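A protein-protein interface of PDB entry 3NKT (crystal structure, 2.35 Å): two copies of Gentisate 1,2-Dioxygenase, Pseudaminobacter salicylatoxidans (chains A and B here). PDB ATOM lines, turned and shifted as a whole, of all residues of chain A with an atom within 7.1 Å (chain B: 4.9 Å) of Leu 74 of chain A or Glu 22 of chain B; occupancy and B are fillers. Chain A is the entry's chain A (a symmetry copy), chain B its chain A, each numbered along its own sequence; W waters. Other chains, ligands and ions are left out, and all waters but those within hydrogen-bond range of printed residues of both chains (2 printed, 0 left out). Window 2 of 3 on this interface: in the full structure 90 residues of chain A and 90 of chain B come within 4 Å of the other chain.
OE2 of Glu 73 of chain A lies within salt-bridge range of NZ of Lys 70 of chain A, 3.9 Å away.
OG1 of Thr 20 of chain B sits at hydrogen-bond distance from N of Leu 23 of chain B (3.2 Å).
OG1 of Thr 20 of chain B is in hydrogen-bond range of OE1 of Glu 22 of chain B, 3.3 Å away.
Leu 26 of chain B touches Lys 70 of chain A.
Leu 26 of chain B touches Ser 71 of chain A.
Leu 74 of chain A touches Pro 17 of chain B.
Leu 74 of chain A touches Glu 22 of chain B (CD1 to O, 3.9 Å).
Leu 23 of chain B touches Leu 74 of chain A (CA to CD1, 3.8 Å).
CD2 of Leu 26 of chain B touches CD1 of Leu 74 of chain A (3.7 Å).
Of chain A, only Leu 74 comes within 4 Å of Glu 22 of chain B.
Of the printed residues of chain B, Lys 70 of chain A touches Leu 26 (3.6 Å).
Of the printed residues of chain A, Pro 17 of chain B touches Leu 74.
Thr 20 of chain B touches none of the printed residues of chain A.
The nearest residue of chain B that does not touch Leu 74 of chain A is Lys 18 of chain B (4.5 Å).
The nearest residue of chain A that does not touch Glu 22 of chain B is Lys 70 of chain A (5.6 Å).
The nearest printed residue of chain A that does not touch Leu 26 of chain B is Val 75 of chain A (4.8 Å).
Of the 9 printed residues of chain B, 4 touch a printed residue of chain A.
Of the 9 printed residues of chain A, 3 touch a printed residue of chain B.
Hydrophobic or aromatic side chains of chain A that line the printed part of chain B: Leu 74.
Along chain A the printed residues that touch a printed residue of chain B span positions 70 to 74.
Among the printed residues, no Asp or Glu carboxylate lies within 4 Å of a Lys or Arg side-chain nitrogen of the other chain.
No position is printed for both chains.
Water W1 bridges O of Leu 74 of chain A (2.8 Å) and N of Lys 18 of chain B (3.2 Å).
Water W2 bridges the backbone carbonyl oxygen of Lys 18 of chain B (3.0 Å) and the backbone carbonyl oxygen of Leu 74 of chain A (3.5 Å).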
ATOM      1  N   ARG A  69       1.138   5.966   5.415  1.00  0.00           N
ATOM      2  CA  ARG A  69       0.865   7.096   4.523  1.00  0.00           C
ATOM      3  C   ARG A  69      -0.067   8.170   5.116  1.00  0.00           C
ATOM      4  O   ARG A  69       0.163   9.378   4.950  1.00  0.00           O
ATOM      5  CB  ARG A  69       0.289   6.606   3.207  1.00  0.00           C
ATOM      6  CG  ARG A  69       1.331   5.983   2.305  1.00  0.00           C
ATOM      7  CD  ARG A  69       0.701   5.533   0.997  1.00  0.00           C
ATOM      8  NE  ARG A  69       1.684   4.885   0.149  1.00  0.00           N
ATOM      9  CZ  ARG A  69       1.413   3.900  -0.711  1.00  0.00           C
ATOM     10  NH1 ARG A  69       0.173   3.427  -0.829  1.00  0.00           N
ATOM     11  NH2 ARG A  69       2.397   3.371  -1.439  1.00  0.00           N
ATOM     12  N   LYS A  70      -1.113   7.726   5.786  1.00  0.00           N
ATOM     13  CA  LYS A  70      -1.993   8.635   6.476  1.00  0.00           C
ATOM     14  C   LYS A  70      -1.250   9.307   7.624  1.00  0.00           C
ATOM     15  O   LYS A  70      -1.381  10.511   7.800  1.00  0.00           O
ATOM     16  CB  LYS A  70      -3.278   7.919   6.949  1.00  0.00           C
ATOM     17  CG  LYS A  70      -4.493   8.847   7.165  1.00  0.00           C
ATOM     18  CD  LYS A  70      -4.529   9.989   6.132  1.00  0.00           C
ATOM     19  CE  LYS A  70      -5.917  10.439   5.792  1.00  0.00           C
ATOM     20  NZ  LYS A  70      -6.315  10.117   4.388  1.00  0.00           N
ATOM     21  N   SER A  71      -0.480   8.537   8.392  1.00  0.00           N
ATOM     22  CA  SER A  71       0.415   9.076   9.409  1.00  0.00           C
ATOM     23  C   SER A  71       1.321  10.121   8.822  1.00  0.00           C
ATOM     24  O   SER A  71       1.583  11.099   9.454  1.00  0.00           O
ATOM     25  CB  SER A  71       1.279   7.980  10.040  1.00  0.00           C
ATOM     26  OG  SER A  71       0.510   7.187  10.926  1.00  0.00           O
ATOM     27  N   GLY A  72       1.800   9.907   7.606  1.00  0.00           N
ATOM     28  CA  GLY A  72       2.610  10.912   6.909  1.00  0.00           C
ATOM     29  C   GLY A  72       1.944  12.250   6.588  1.00  0.00           C
ATOM     30  O   GLY A  72       2.627  13.261   6.479  1.00  0.00           O
ATOM     31  N   GLU A  73       0.623  12.271   6.427  1.00  0.00           N
ATOM     32  CA  GLU A  73      -0.124  13.528   6.258  1.00  0.00           C
ATOM     33  C   GLU A  73      -0.365  14.270   7.568  1.00  0.00           C
ATOM     34  O   GLU A  73      -0.300  15.504   7.624  1.00  0.00           O
ATOM     35  CB  GLU A  73      -1.499  13.255   5.665  1.00  0.00           C
ATOM     36  CG  GLU A  73      -1.499  12.808   4.210  1.00  0.00           C
ATOM     37  CD  GLU A  73      -2.921  12.513   3.729  1.00  0.00           C
ATOM     38  OE1 GLU A  73      -3.896  13.184   4.186  1.00  0.00           O
ATOM     39  OE2 GLU A  73      -3.052  11.594   2.900  1.00  0.00           O
ATOM     40  N   LEU A  74      -0.657  13.510   8.620  1.00  0.00           N
ATOM     41  CA  LEU A  74      -1.231  14.093   9.837  1.00  0.00           C
ATOM     42  C   LEU A  74      -0.233  14.347  10.937  1.00  0.00           C
ATOM     43  O   LEU A  74      -0.507  15.128  11.867  1.00  0.00           O
ATOM     44  CB  LEU A  74      -2.351  13.206  10.379  1.00  0.00           C
ATOM     45  CG  LEU A  74      -3.513  12.945   9.413  1.00  0.00           C
ATOM     46  CD1 LEU A  74      -4.539  12.018  10.073  1.00  0.00           C
ATOM     47  CD2 LEU A  74      -4.204  14.242   8.916  1.00  0.00           C
ATOM     48  N   VAL A  75       0.917  13.683  10.871  1.00  0.00           N
ATOM     49  CA  VAL A  75       1.861  13.764  11.987  1.00  0.00           C
ATOM     50  C   VAL A  75       3.224  14.251  11.514  1.00  0.00           C
ATOM     51  O   VAL A  75       3.823  13.644  10.647  1.00  0.00           O
ATOM     52  CB  VAL A  75       2.020  12.410  12.704  1.00  0.00           C
ATOM     53  CG1 VAL A  75       2.900  12.570  13.985  1.00  0.00           C
ATOM     54  CG2 VAL A  75       0.666  11.791  13.006  1.00  0.00           C
ATOM     55  N   PRO A  76       3.719  15.350  12.090  1.00  0.00           N
ATOM     56  CA  PRO A  76       5.067  15.726  11.676  1.00  0.00           C
ATOM     57  C   PRO A  76       6.095  14.840  12.379  1.00  0.00           C
ATOM     58  O   PRO A  76       5.867  14.382  13.493  1.00  0.00           O
ATOM     59  CB  PRO A  76       5.198  17.174  12.140  1.00  0.00           C
ATOM     60  CG  PRO A  76       4.293  17.260  13.340  1.00  0.00           C
ATOM     61  CD  PRO A  76       3.157  16.262  13.102  1.00  0.00           C
ATOM     62  N   ARG A  84       8.363   8.706  12.845  1.00  0.00           N
ATOM     63  CA  ARG A  84       7.049   8.286  12.389  1.00  0.00           C
ATOM     64  C   ARG A  84       7.067   6.791  12.132  1.00  0.00           C
ATOM     65  O   ARG A  84       7.088   6.328  11.016  1.00  0.00           O
ATOM     66  CB  ARG A  84       6.613   9.042  11.148  1.00  0.00           C
ATOM     67  CG  ARG A  84       5.137   9.046  10.920  1.00  0.00           C
ATOM     68  CD  ARG A  84       4.716  10.234  10.138  1.00  0.00           C
ATOM     69  NE  ARG A  84       5.719  10.491   9.160  1.00  0.00           N
ATOM     70  CZ  ARG A  84       6.211  11.662   8.849  1.00  0.00           C
ATOM     71  NH1 ARG A  84       5.769  12.760   9.390  1.00  0.00           N
ATOM     72  NH2 ARG A  84       7.153  11.703   7.959  1.00  0.00           N
ATOM     73  N   PRO B  17       0.463  15.905  16.862  1.00  0.00           N
ATOM     74  CA  PRO B  17      -0.365  16.236  15.697  1.00  0.00           C
ATOM     75  C   PRO B  17      -1.604  17.082  16.066  1.00  0.00           C
ATOM     76  O   PRO B  17      -2.006  17.118  17.250  1.00  0.00           O
ATOM     77  CB  PRO B  17      -0.770  14.863  15.153  1.00  0.00           C
ATOM     78  CG  PRO B  17      -0.717  13.970  16.323  1.00  0.00           C
ATOM     79  CD  PRO B  17       0.145  14.580  17.406  1.00  0.00           C
ATOM     80  N   LYS B  18      -2.193  17.763  15.081  1.00  0.00           N
ATOM     81  CA  LYS B  18      -3.430  18.522  15.332  1.00  0.00           C
ATOM     82  C   LYS B  18      -4.602  17.585  15.696  1.00  0.00           C
ATOM     83  O   LYS B  18      -4.866  16.656  14.961  1.00  0.00           O
ATOM     84  CB  LYS B  18      -3.774  19.387  14.129  1.00  0.00           C
ATOM     85  CG  LYS B  18      -2.847  20.567  13.955  1.00  0.00           C
ATOM     86  CD  LYS B  18      -3.344  21.485  12.851  1.00  0.00           C
ATOM     87  CE  LYS B  18      -2.324  22.596  12.576  1.00  0.00           C
ATOM     88  NZ  LYS B  18      -2.567  23.142  11.225  1.00  0.00           N
ATOM     89  N   THR B  20      -7.717  16.529  15.336  1.00  0.00           N
ATOM     90  CA  THR B  20      -8.856  16.681  14.423  1.00  0.00           C
ATOM     91  C   THR B  20      -9.652  15.373  14.349  1.00  0.00           C
ATOM     92  O   THR B  20      -9.161  14.363  14.801  1.00  0.00           O
ATOM     93  CB  THR B  20      -8.363  17.034  13.004  1.00  0.00           C
ATOM     94  OG1 THR B  20      -7.502  15.991  12.534  1.00  0.00           O
ATOM     95  CG2 THR B  20      -7.585  18.398  12.970  1.00  0.00           C
ATOM     96  N   PRO B  21     -10.873  15.376  13.758  1.00  0.00           N
ATOM     97  CA  PRO B  21     -11.587  14.079  13.587  1.00  0.00           C
ATOM     98  C   PRO B  21     -10.823  13.050  12.722  1.00  0.00           C
ATOM     99  O   PRO B  21     -10.974  11.868  12.908  1.00  0.00           O
ATOM    100  CB  PRO B  21     -12.904  14.477  12.871  1.00  0.00           C
ATOM    101  CG  PRO B  21     -13.050  15.999  13.135  1.00  0.00           C
ATOM    102  CD  PRO B  21     -11.652  16.520  13.226  1.00  0.00           C
ATOM    103  N   GLU B  22     -10.013  13.498  11.785  1.00  0.00           N
ATOM    104  CA  GLU B  22      -9.270  12.571  10.963  1.00  0.00           C
ATOM    105  C   GLU B  22      -8.118  11.947  11.778  1.00  0.00           C
ATOM    106  O   GLU B  22      -7.877  10.732  11.703  1.00  0.00           O
ATOM    107  CB  GLU B  22      -8.752  13.259   9.702  1.00  0.00           C
ATOM    108  CG  GLU B  22      -9.822  13.929   8.821  1.00  0.00           C
ATOM    109  CD  GLU B  22     -10.190  15.376   9.245  1.00  0.00           C
ATOM    110  OE1 GLU B  22      -9.994  15.755  10.419  1.00  0.00           O
ATOM    111  OE2 GLU B  22     -10.695  16.143   8.398  1.00  0.00           O
ATOM    112  N   LEU B  23      -7.419  12.755  12.568  1.00  0.00           N
ATOM    113  CA  LEU B  23      -6.395  12.188  13.422  1.00  0.00           C
ATOM    114  C   LEU B  23      -7.021  11.117  14.340  1.00  0.00           C
ATOM    115  O   LEU B  23      -6.487  10.012  14.457  1.00  0.00           O
ATOM    116  CB  LEU B  23      -5.612  13.243  14.214  1.00  0.00           C
ATOM    117  CG  LEU B  23      -4.578  12.544  15.119  1.00  0.00           C
ATOM    118  CD1 LEU B  23      -3.281  12.233  14.333  1.00  0.00           C
ATOM    119  CD2 LEU B  23      -4.331  13.300  16.420  1.00  0.00           C
ATOM    120  N   ARG B  24      -8.167  11.439  14.942  1.00  0.00           N
ATOM    121  CA  ARG B  24      -8.844  10.529  15.877  1.00  0.00           C
ATOM    122  C   ARG B  24      -9.273   9.238  15.166  1.00  0.00           C
ATOM    123  O   ARG B  24      -9.153   8.164  15.741  1.00  0.00           O
ATOM    124  CB  ARG B  24     -10.039  11.222  16.561  1.00  0.00           C
ATOM    125  CG  ARG B  24      -9.801  11.664  17.986  1.00  0.00           C
ATOM    126  CD  ARG B  24     -10.996  12.476  18.518  1.00  0.00           C
ATOM    127  NE  ARG B  24     -10.669  13.872  18.310  1.00  0.00           N
ATOM    128  CZ  ARG B  24     -11.353  14.767  17.602  1.00  0.00           C
ATOM    129  NH1 ARG B  24     -12.500  14.497  17.011  1.00  0.00           N
ATOM    130  NH2 ARG B  24     -10.844  15.975  17.503  1.00  0.00           N
ATOM    131  N   ALA B  25      -9.744   9.359  13.923  1.00  0.00           N
ATOM    132  CA  ALA B  25     -10.050   8.224  13.073  1.00  0.00           C
ATOM    133  C   ALA B  25      -8.805   7.365  12.753  1.00  0.00           C
ATOM    134  O   ALA B  25      -8.901   6.147  12.644  1.00  0.00           O
ATOM    135  CB  ALA B  25     -10.747   8.682  11.764  1.00  0.00           C
ATOM    136  N   LEU B  26      -7.661   8.020  12.559  1.00  0.00           N
ATOM    137  CA  LEU B  26      -6.420   7.327  12.252  1.00  0.00           C
ATOM    138  C   LEU B  26      -6.007   6.531  13.477  1.00  0.00           C
ATOM    139  O   LEU B  26      -5.543   5.411  13.322  1.00  0.00           O
ATOM    140  CB  LEU B  26      -5.319   8.315  11.817  1.00  0.00           C
ATOM    141  CG  LEU B  26      -3.882   7.819  11.595  1.00  0.00           C
ATOM    142  CD1 LEU B  26      -3.817   6.902  10.367  1.00  0.00           C
ATOM    143  CD2 LEU B  26      -2.887   8.949  11.447  1.00  0.00           C
HETATM  144  O   HOH W   1      -1.338  17.797  12.039  1.00  0.00           O
HETATM  145  O   HOH W   2      -3.819  16.187  12.177  1.00  0.00           O
